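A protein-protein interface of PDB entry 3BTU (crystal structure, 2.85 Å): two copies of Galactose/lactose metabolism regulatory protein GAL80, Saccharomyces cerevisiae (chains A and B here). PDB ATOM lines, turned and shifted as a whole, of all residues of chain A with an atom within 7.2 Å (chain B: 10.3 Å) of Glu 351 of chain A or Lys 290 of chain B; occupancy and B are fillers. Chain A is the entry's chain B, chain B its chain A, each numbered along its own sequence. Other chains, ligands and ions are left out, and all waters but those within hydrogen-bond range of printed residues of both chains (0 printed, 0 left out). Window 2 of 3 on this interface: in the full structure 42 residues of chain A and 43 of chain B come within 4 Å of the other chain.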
ATOM      1  N   ASP A 298      24.345   5.683  19.527  1.00  0.00           N
ATOM      2  CA  ASP A 298      23.309   5.392  18.540  1.00  0.00           C
ATOM      3  C   ASP A 298      23.916   5.245  17.148  1.00  0.00           C
ATOM      4  O   ASP A 298      24.093   6.235  16.450  1.00  0.00           O
ATOM      5  CB  ASP A 298      22.281   6.526  18.540  1.00  0.00           C
ATOM      6  CG  ASP A 298      20.867   6.047  18.248  1.00  0.00           C
ATOM      7  OD1 ASP A 298      20.676   4.836  18.001  1.00  0.00           O
ATOM      8  OD2 ASP A 298      19.937   6.886  18.277  1.00  0.00           O
ATOM      9  N   HIS A 300      23.816   4.084  13.217  1.00  0.00           N
ATOM     10  CA  HIS A 300      22.783   3.821  12.206  1.00  0.00           C
ATOM     11  C   HIS A 300      23.336   3.267  10.905  1.00  0.00           C
ATOM     12  O   HIS A 300      24.177   3.899  10.262  1.00  0.00           O
ATOM     13  CB  HIS A 300      21.975   5.079  11.918  1.00  0.00           C
ATOM     14  CG  HIS A 300      21.469   5.754  13.148  1.00  0.00           C
ATOM     15  ND1 HIS A 300      20.452   5.229  13.914  1.00  0.00           N
ATOM     16  CD2 HIS A 300      21.845   6.906  13.754  1.00  0.00           C
ATOM     17  CE1 HIS A 300      20.227   6.026  14.946  1.00  0.00           C
ATOM     18  NE2 HIS A 300      21.054   7.053  14.868  1.00  0.00           N
ATOM     19  N   GLY A 301      22.844   2.096  10.502  1.00  0.00           N
ATOM     20  CA  GLY A 301      23.338   1.451   9.293  1.00  0.00           C
ATOM     21  C   GLY A 301      22.340   1.391   8.147  1.00  0.00           C
ATOM     22  O   GLY A 301      21.206   1.855   8.248  1.00  0.00           O
ATOM     23  N   THR A 302      22.775   0.796   7.047  1.00  0.00           N
ATOM     24  CA  THR A 302      21.953   0.697   5.852  1.00  0.00           C
ATOM     25  C   THR A 302      21.026  -0.502   5.938  1.00  0.00           C
ATOM     26  O   THR A 302      19.917  -0.476   5.397  1.00  0.00           O
ATOM     27  CB  THR A 302      22.810   0.567   4.595  1.00  0.00           C
ATOM     28  OG1 THR A 302      23.588  -0.634   4.678  1.00  0.00           O
ATOM     29  CG2 THR A 302      23.735   1.768   4.449  1.00  0.00           C
ATOM     30  N   LYS A 303      21.478  -1.555   6.611  1.00  0.00           N
ATOM     31  CA  LYS A 303      20.645  -2.742   6.828  1.00  0.00           C
ATOM     32  C   LYS A 303      20.113  -2.825   8.257  1.00  0.00           C
ATOM     33  O   LYS A 303      19.371  -3.746   8.588  1.00  0.00           O
ATOM     34  CB  LYS A 303      21.414  -4.030   6.520  1.00  0.00           C
ATOM     35  CG  LYS A 303      22.045  -4.106   5.145  1.00  0.00           C
ATOM     36  CD  LYS A 303      22.635  -5.489   4.926  1.00  0.00           C
ATOM     37  CE  LYS A 303      23.646  -5.498   3.792  1.00  0.00           C
ATOM     38  NZ  LYS A 303      24.298  -6.839   3.655  1.00  0.00           N
ATOM     39  N   GLY A 304      20.498  -1.880   9.108  1.00  0.00           N
ATOM     40  CA  GLY A 304      20.040  -1.906  10.486  1.00  0.00           C
ATOM     41  C   GLY A 304      20.623  -0.847  11.404  1.00  0.00           C
ATOM     42  O   GLY A 304      21.511  -0.093  11.020  1.00  0.00           O
ATOM     43  N   ASP A 305      20.100  -0.789  12.624  1.00  0.00           N
ATOM     44  CA  ASP A 305      20.602   0.111  13.651  1.00  0.00           C
ATOM     45  C   ASP A 305      21.244  -0.699  14.754  1.00  0.00           C
ATOM     46  O   ASP A 305      21.128  -1.920  14.782  1.00  0.00           O
ATOM     47  CB  ASP A 305      19.474   0.929  14.259  1.00  0.00           C
ATOM     48  CG  ASP A 305      19.213   2.206  13.509  1.00  0.00           C
ATOM     49  OD1 ASP A 305      19.604   2.292  12.320  1.00  0.00           O
ATOM     50  OD2 ASP A 305      18.612   3.125  14.113  1.00  0.00           O
ATOM     51  N   LEU A 306      21.895  -0.015  15.683  1.00  0.00           N
ATOM     52  CA  LEU A 306      22.558  -0.669  16.796  1.00  0.00           C
ATOM     53  C   LEU A 306      22.764   0.395  17.857  1.00  0.00           C
ATOM     54  O   LEU A 306      23.355   1.435  17.578  1.00  0.00           O
ATOM     55  CB  LEU A 306      23.884  -1.252  16.325  1.00  0.00           C
ATOM     56  CG  LEU A 306      24.601  -2.255  17.219  1.00  0.00           C
ATOM     57  CD1 LEU A 306      25.699  -2.962  16.442  1.00  0.00           C
ATOM     58  CD2 LEU A 306      25.200  -1.544  18.409  1.00  0.00           C
ATOM     59  N   LYS A 307      22.267   0.157  19.066  1.00  0.00           N
ATOM     60  CA  LYS A 307      22.299   1.194  20.104  1.00  0.00           C
ATOM     61  C   LYS A 307      22.656   0.672  21.510  1.00  0.00           C
ATOM     62  O   LYS A 307      22.125  -0.352  21.963  1.00  0.00           O
ATOM     63  CB  LYS A 307      20.967   1.961  20.137  1.00  0.00           C
ATOM     64  CG  LYS A 307      20.751   2.754  21.416  1.00  0.00           C
ATOM     65  CD  LYS A 307      19.315   3.221  21.578  1.00  0.00           C
ATOM     66  CE  LYS A 307      19.166   4.696  21.271  1.00  0.00           C
ATOM     67  NZ  LYS A 307      17.863   5.253  21.756  1.00  0.00           N
ATOM     68  N   TYR A 324      19.786  -4.043  18.665  1.00  0.00           N
ATOM     69  CA  TYR A 324      20.290  -4.067  17.281  1.00  0.00           C
ATOM     70  C   TYR A 324      19.372  -4.634  16.204  1.00  0.00           C
ATOM     71  O   TYR A 324      19.200  -5.844  16.119  1.00  0.00           O
ATOM     72  CB  TYR A 324      21.663  -4.731  17.206  1.00  0.00           C
ATOM     73  CG  TYR A 324      21.726  -6.145  17.713  1.00  0.00           C
ATOM     74  CD1 TYR A 324      21.622  -7.226  16.838  1.00  0.00           C
ATOM     75  CD2 TYR A 324      21.937  -6.408  19.066  1.00  0.00           C
ATOM     76  CE1 TYR A 324      21.700  -8.541  17.309  1.00  0.00           C
ATOM     77  CE2 TYR A 324      22.021  -7.718  19.549  1.00  0.00           C
ATOM     78  CZ  TYR A 324      21.900  -8.782  18.670  1.00  0.00           C
ATOM     79  OH  TYR A 324      21.975 -10.079  19.149  1.00  0.00           O
ATOM     80  N   SER A 325      18.860  -3.753  15.340  1.00  0.00           N
ATOM     81  CA  SER A 325      17.723  -4.053  14.439  1.00  0.00           C
ATOM     82  C   SER A 325      17.973  -5.035  13.302  1.00  0.00           C
ATOM     83  O   SER A 325      19.066  -5.547  13.158  1.00  0.00           O
ATOM     84  CB  SER A 325      17.163  -2.778  13.859  1.00  0.00           C
ATOM     85  OG  SER A 325      18.074  -2.330  12.885  1.00  0.00           O
ATOM     86  N   LYS A 350      11.057  -6.530   7.455  1.00  0.00           N
ATOM     87  CA  LYS A 350      10.946  -7.966   7.393  1.00  0.00           C
ATOM     88  C   LYS A 350      12.096  -7.910   8.433  1.00  0.00           C
ATOM     89  O   LYS A 350      13.169  -8.507   8.286  1.00  0.00           O
ATOM     90  CB  LYS A 350      11.439  -8.645   6.127  1.00  0.00           C
ATOM     91  CG  LYS A 350      11.600 -10.187   6.352  1.00  0.00           C
ATOM     92  CD  LYS A 350      11.817 -10.557   7.866  1.00  0.00           C
ATOM     93  CE  LYS A 350      12.336 -11.971   8.140  1.00  0.00           C
ATOM     94  NZ  LYS A 350      11.228 -12.926   8.488  1.00  0.00           N
ATOM     95  N   GLU A 351      11.857  -7.079   9.446  1.00  0.00           N
ATOM     96  CA  GLU A 351      12.861  -6.638  10.400  1.00  0.00           C
ATOM     97  C   GLU A 351      12.861  -7.498  11.643  1.00  0.00           C
ATOM     98  O   GLU A 351      11.810  -7.883  12.144  1.00  0.00           O
ATOM     99  CB  GLU A 351      12.588  -5.184  10.800  1.00  0.00           C
ATOM    100  CG  GLU A 351      13.305  -4.153   9.937  1.00  0.00           C
ATOM    101  CD  GLU A 351      12.407  -2.989   9.498  1.00  0.00           C
ATOM    102  OE1 GLU A 351      11.282  -3.251   8.996  1.00  0.00           O
ATOM    103  OE2 GLU A 351      12.839  -1.815   9.634  1.00  0.00           O
ATOM    104  N   ILE A 352      14.050  -7.788  12.148  1.00  0.00           N
ATOM    105  CA  ILE A 352      14.176  -8.518  13.395  1.00  0.00           C
ATOM    106  C   ILE A 352      14.942  -7.712  14.429  1.00  0.00           C
ATOM    107  O   ILE A 352      16.128  -7.461  14.268  1.00  0.00           O
ATOM    108  CB  ILE A 352      14.866  -9.870  13.187  1.00  0.00           C
ATOM    109  CG1 ILE A 352      13.811 -10.931  12.866  1.00  0.00           C
ATOM    110  CG2 ILE A 352      15.666 -10.251  14.421  1.00  0.00           C
ATOM    111  CD1 ILE A 352      14.028 -12.267  13.564  1.00  0.00           C
ATOM    112  N   MET A 353      14.260  -7.301  15.489  1.00  0.00           N
ATOM    113  CA  MET A 353      14.923  -6.567  16.555  1.00  0.00           C
ATOM    114  C   MET A 353      15.343  -7.486  17.687  1.00  0.00           C
ATOM    115  O   MET A 353      14.682  -8.486  17.976  1.00  0.00           O
ATOM    116  CB  MET A 353      14.028  -5.454  17.075  1.00  0.00           C
ATOM    117  CG  MET A 353      13.754  -4.403  16.041  1.00  0.00           C
ATOM    118  SD  MET A 353      12.482  -3.234  16.555  1.00  0.00           S
ATOM    119  CE  MET A 353      12.704  -1.937  15.315  1.00  0.00           C
ATOM    120  N   ASN B 184      15.087  14.621  10.565  1.00  0.00           N
ATOM    121  CA  ASN B 184      15.181  13.872   9.330  1.00  0.00           C
ATOM    122  C   ASN B 184      14.634  14.633   8.136  1.00  0.00           C
ATOM    123  O   ASN B 184      13.499  15.098   8.161  1.00  0.00           O
ATOM    124  CB  ASN B 184      14.468  12.547   9.475  1.00  0.00           C
ATOM    125  CG  ASN B 184      14.958  11.532   8.484  1.00  0.00           C
ATOM    126  OD1 ASN B 184      14.838  11.731   7.267  1.00  0.00           O
ATOM    127  ND2 ASN B 184      15.530  10.434   8.989  1.00  0.00           N
ATOM    128  N   TYR B 190      19.004   6.710   0.742  1.00  0.00           N
ATOM    129  CA  TYR B 190      19.663   5.965  -0.328  1.00  0.00           C
ATOM    130  C   TYR B 190      18.769   5.754  -1.553  1.00  0.00           C
ATOM    131  O   TYR B 190      19.257   5.493  -2.655  1.00  0.00           O
ATOM    132  CB  TYR B 190      20.179   4.623   0.202  1.00  0.00           C
ATOM    133  CG  TYR B 190      21.250   4.782   1.246  1.00  0.00           C
ATOM    134  CD1 TYR B 190      20.927   5.003   2.580  1.00  0.00           C
ATOM    135  CD2 TYR B 190      22.594   4.733   0.899  1.00  0.00           C
ATOM    136  CE1 TYR B 190      21.918   5.163   3.539  1.00  0.00           C
ATOM    137  CE2 TYR B 190      23.587   4.889   1.844  1.00  0.00           C
ATOM    138  CZ  TYR B 190      23.250   5.104   3.162  1.00  0.00           C
ATOM    139  OH  TYR B 190      24.251   5.257   4.106  1.00  0.00           O
ATOM    140  N   LYS B 283      19.522  13.649   9.757  1.00  0.00           N
ATOM    141  CA  LYS B 283      19.683  12.511   8.849  1.00  0.00           C
ATOM    142  C   LYS B 283      19.005  12.786   7.493  1.00  0.00           C
ATOM    143  O   LYS B 283      17.909  13.345   7.443  1.00  0.00           O
ATOM    144  CB  LYS B 283      19.093  11.258   9.491  1.00  0.00           C
ATOM    145  CG  LYS B 283      19.710   9.947   9.054  1.00  0.00           C
ATOM    146  CD  LYS B 283      19.138   8.788   9.869  1.00  0.00           C
ATOM    147  CE  LYS B 283      19.689   7.438   9.435  1.00  0.00           C
ATOM    148  NZ  LYS B 283      19.258   7.044   8.073  1.00  0.00           N
ATOM    149  N   GLY B 285      17.588  10.819   5.132  1.00  0.00           N
ATOM    150  CA  GLY B 285      16.291  10.178   5.016  1.00  0.00           C
ATOM    151  C   GLY B 285      16.329   8.770   5.570  1.00  0.00           C
ATOM    152  O   GLY B 285      16.827   8.534   6.673  1.00  0.00           O
ATOM    153  N   LYS B 286      15.819   7.825   4.796  1.00  0.00           N
ATOM    154  CA  LYS B 286      15.687   6.453   5.255  1.00  0.00           C
ATOM    155  C   LYS B 286      17.030   5.738   5.204  1.00  0.00           C
ATOM    156  O   LYS B 286      17.959   6.215   4.565  1.00  0.00           O
ATOM    157  CB  LYS B 286      14.648   5.719   4.411  1.00  0.00           C
ATOM    158  CG  LYS B 286      13.284   6.404   4.383  1.00  0.00           C
ATOM    159  CD  LYS B 286      12.254   5.560   3.641  1.00  0.00           C
ATOM    160  CE  LYS B 286      10.835   6.037   3.912  1.00  0.00           C
ATOM    161  NZ  LYS B 286       9.834   4.966   3.601  1.00  0.00           N
ATOM    162  N   PRO B 287      17.154   4.606   5.908  1.00  0.00           N
ATOM    163  CA  PRO B 287      16.124   4.052   6.791  1.00  0.00           C
ATOM    164  C   PRO B 287      15.851   4.998   7.953  1.00  0.00           C
ATOM    165  O   PRO B 287      16.680   5.856   8.225  1.00  0.00           O
ATOM    166  CB  PRO B 287      16.774   2.769   7.318  1.00  0.00           C
ATOM    167  CG  PRO B 287      17.817   2.428   6.311  1.00  0.00           C
ATOM    168  CD  PRO B 287      18.337   3.737   5.827  1.00  0.00           C
ATOM    169  N   THR B 288      14.705   4.871   8.614  1.00  0.00           N
ATOM    170  CA  THR B 288      14.459   5.678   9.797  1.00  0.00           C
ATOM    171  C   THR B 288      15.245   5.065  10.916  1.00  0.00           C
ATOM    172  O   THR B 288      15.782   3.966  10.769  1.00  0.00           O
ATOM    173  CB  THR B 288      12.981   5.680  10.205  1.00  0.00           C
ATOM    174  OG1 THR B 288      12.584   4.357  10.597  1.00  0.00           O
ATOM    175  CG2 THR B 288      12.124   6.194   9.045  1.00  0.00           C
ATOM    176  N   LYS B 289      15.307   5.769  12.041  1.00  0.00           N
ATOM    177  CA  LYS B 289      15.948   5.233  13.234  1.00  0.00           C
ATOM    178  C   LYS B 289      15.063   4.174  13.896  1.00  0.00           C
ATOM    179  O   LYS B 289      13.883   4.407  14.165  1.00  0.00           O
ATOM    180  CB  LYS B 289      16.313   6.368  14.194  1.00  0.00           C
ATOM    181  CG  LYS B 289      17.475   7.214  13.679  1.00  0.00           C
ATOM    182  CD  LYS B 289      18.028   8.189  14.719  1.00  0.00           C
ATOM    183  CE  LYS B 289      17.756   9.649  14.353  1.00  0.00           C
ATOM    184  NZ  LYS B 289      18.578  10.550  15.225  1.00  0.00           N
ATOM    185  N   LYS B 290      15.647   3.004  14.133  1.00  0.00           N
ATOM    186  CA  LYS B 290      14.928   1.867  14.706  1.00  0.00           C
ATOM    187  C   LYS B 290      14.700   1.974  16.214  1.00  0.00           C
ATOM    188  O   LYS B 290      13.702   1.482  16.726  1.00  0.00           O
ATOM    189  CB  LYS B 290      15.658   0.554  14.414  1.00  0.00           C
ATOM    190  CG  LYS B 290      16.139   0.394  12.988  1.00  0.00           C
ATOM    191  CD  LYS B 290      15.036   0.581  11.981  1.00  0.00           C
ATOM    192  CE  LYS B 290      15.572   0.467  10.565  1.00  0.00           C
ATOM    193  NZ  LYS B 290      14.571   0.969   9.581  1.00  0.00           N
ATOM    194  N   PHE B 291      15.612   2.606  16.932  1.00  0.00           N
ATOM    195  CA  PHE B 291      15.469   2.650  18.383  1.00  0.00           C
ATOM    196  C   PHE B 291      15.386   4.058  18.972  1.00  0.00           C
ATOM    197  O   PHE B 291      15.638   4.246  20.159  1.00  0.00           O
ATOM    198  CB  PHE B 291      16.598   1.870  19.074  1.00  0.00           C
ATOM    199  CG  PHE B 291      16.722   0.452  18.614  1.00  0.00           C
ATOM    200  CD1 PHE B 291      17.742   0.078  17.770  1.00  0.00           C
ATOM    201  CD2 PHE B 291      15.814  -0.503  19.023  1.00  0.00           C
ATOM    202  CE1 PHE B 291      17.864  -1.224  17.346  1.00  0.00           C
ATOM    203  CE2 PHE B 291      15.929  -1.803  18.602  1.00  0.00           C
ATOM    204  CZ  PHE B 291      16.958  -2.167  17.764  1.00  0.00           C
ATOM    205  N   THR B 292      15.036   5.043  18.158  1.00  0.00           N
ATOM    206  CA  THR B 292      14.911   6.403  18.658  1.00  0.00           C
ATOM    207  C   THR B 292      13.879   7.140  17.818  1.00  0.00           C
ATOM    208  O   THR B 292      13.717   6.830  16.644  1.00  0.00           O
ATOM    209  CB  THR B 292      16.265   7.132  18.569  1.00  0.00           C
ATOM    210  OG1 THR B 292      17.284   6.336  19.204  1.00  0.00           O
ATOM    211  CG2 THR B 292      16.186   8.492  19.235  1.00  0.00           C
ATOM    212  N   LYS B 293      13.154   8.084  18.406  1.00  0.00           N
ATOM    213  CA  LYS B 293      12.243   8.873  17.600  1.00  0.00           C
ATOM    214  C   LYS B 293      13.066   9.603  16.545  1.00  0.00           C
ATOM    215  O   LYS B 293      14.245   9.898  16.777  1.00  0.00           O
ATOM    216  CB  LYS B 293      11.456   9.859  18.454  1.00  0.00           C
ATOM    217  CG  LYS B 293      10.470   9.212  19.393  1.00  0.00           C
ATOM    218  CD  LYS B 293       9.442   8.392  18.657  1.00  0.00           C
ATOM    219  CE  LYS B 293       8.428   7.821  19.635  1.00  0.00           C
ATOM    220  NZ  LYS B 293       7.384   6.986  18.979  1.00  0.00           N
ATOM    221  N   ASN B 294      12.458   9.878  15.389  1.00  0.00           N
ATOM    222  CA  ASN B 294      13.160  10.522  14.288  1.00  0.00           C
ATOM    223  C   ASN B 294      13.232  12.024  14.450  1.00  0.00           C
ATOM    224  O   ASN B 294      14.084  12.673  13.853  1.00  0.00           O
ATOM    225  CB  ASN B 294      12.535  10.154  12.941  1.00  0.00           C
ATOM    226  CG  ASN B 294      12.856   8.725  12.513  1.00  0.00           C
ATOM    227  OD1 ASN B 294      14.024   8.341  12.415  1.00  0.00           O
ATOM    228  ND2 ASN B 294      11.820   7.936  12.248  1.00  0.00           N
ATOM    229  N   LEU B 295      12.348  12.586  15.259  1.00  0.00           N
ATOM    230  CA  LEU B 295      12.517  13.979  15.657  1.00  0.00           C
ATOM    231  C   LEU B 295      12.586  14.092  17.167  1.00  0.00           C
ATOM    232  O   LEU B 295      11.740  13.546  17.874  1.00  0.00           O
ATOM    233  CB  LEU B 295      11.394  14.864  15.147  1.00  0.00           C
ATOM    234  CG  LEU B 295      11.502  16.255  15.768  1.00  0.00           C
ATOM    235  CD1 LEU B 295      12.745  16.935  15.260  1.00  0.00           C
ATOM    236  CD2 LEU B 295      10.292  17.095  15.458  1.00  0.00           C
ATOM    237  N   ASP B 311       7.665  11.281  14.963  1.00  0.00           N
ATOM    238  CA  ASP B 311       8.146  10.201  14.115  1.00  0.00           C
ATOM    239  C   ASP B 311       8.373  10.704  12.703  1.00  0.00           C
ATOM    240  O   ASP B 311       8.826   9.960  11.839  1.00  0.00           O
ATOM    241  CB  ASP B 311       7.167   9.032  14.102  1.00  0.00           C
ATOM    242  CG  ASP B 311       6.827   8.532  15.501  1.00  0.00           C
ATOM    243  OD1 ASP B 311       7.289   7.428  15.874  1.00  0.00           O
ATOM    244  OD2 ASP B 311       6.094   9.242  16.227  1.00  0.00           O
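The side-chain amino group of Lys 290 of chain B lies within salt-bridge range of the side-chain carboxylate of Glu 351 of chain A (3.3 Å). N of Lys 290 of chain B lies within hydrogen-bond range of OD2 of Asp 305 of chain A. NZ of Lys 307 of chain A is in hydrogen-bond range of OG1 of Thr 292 of chain B (2.8 Å). The side-chain hydroxyl (OG1) of Thr 292 of chain B lies within hydrogen-bond range of the side-chain carboxylate (OD2) of Asp 298 of chain A (2.9 Å). The backbone carbonyl oxygen of Phe 291 of chain B sits at hydrogen-bond distance from the side-chain amino group of Lys 307 of chain A (2.9 Å).
The side-chain carboxylate (OD2) of Asp 305 of chain A sits at hydrogen-bond distance from a ring nitrogen (ND1) of His 300 of chain A, 2.8 Å away. N of Asp 305 of chain A is in hydrogen-bond range of OG of Ser 325 of chain A. O of Thr 288 of chain B is in hydrogen-bond range of NZ of Lys 290 of chain B (3.4 Å). The side-chain amino group (NZ) of Lys 283 of chain B lies within hydrogen-bond range of the backbone carbonyl oxygen (O) of Pro 287 of chain B (2.8 Å). The backbone NH of Lys 289 of chain B is in hydrogen-bond range of the side-chain amide oxygen of Asn 294 of chain B, at 2.9 Å.
Among the printed residues, pairs that only touch across the chains: His 300 of chain A with Lys 289 of chain B, Gly 301 of chain A with Pro 287 of chain B, Thr 302 of chain A with Tyr 190 of chain B, Thr 302 of chain A with Pro 287 of chain B, Asp 305 of chain A with Lys 289 of chain B, Tyr 324 of chain A with Phe 291 of chain B, Ser 325 of chain A with Lys 290 of chain B, Ser 325 of chain A with Phe 291 of chain B and Met 353 of chain A with Lys 290 of chain B.
Of the printed residues of chain B, His 300 of chain A touches Lys 289. Printed residues of chain B within 4 Å of Gly 301 of chain A: Pro 287. No residue of chain B comes within 4 Å of Lys 350 of chain A. Printed residues of chain B within 4 Å of Glu 351 of chain A: Lys 290 (3.3 Å). No residue of chain B comes within 4 Å of Ile 352 of chain A. Lys 286 of chain B touches none of the printed residues of chain A. Of the printed residues of chain A, Lys 289 of chain B touches His 300 and Asp 305. Of chain A, only Asp 305, Ser 325, Glu 351 and Met 353 come within 4 Å of Lys 290 of chain B. Of the printed residues of chain A, Phe 291 of chain B touches Lys 307 (2.9 Å), Tyr 324 (3.5 Å) and Ser 325 (3.4 Å). The nearest residue of chain B that does not touch Glu 351 of chain A is Thr 288 of chain B (6.3 Å). The nearest residue of chain A that does not touch Lys 290 of chain B is Gly 304 of chain A (4.9 Å). The nearest printed residue of chain B that does not touch His 300 of chain A is Lys 283 of chain B (4.1 Å).
Of the 15 printed residues of chain B, 6 touch a printed residue of chain A. Among the printed residues, 14 pairs touch across the chains.
No position is printed for both chains. Of the 14 pairs that touch across the chains among the printed residues, none has its exchanged pair printed and touching as well.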
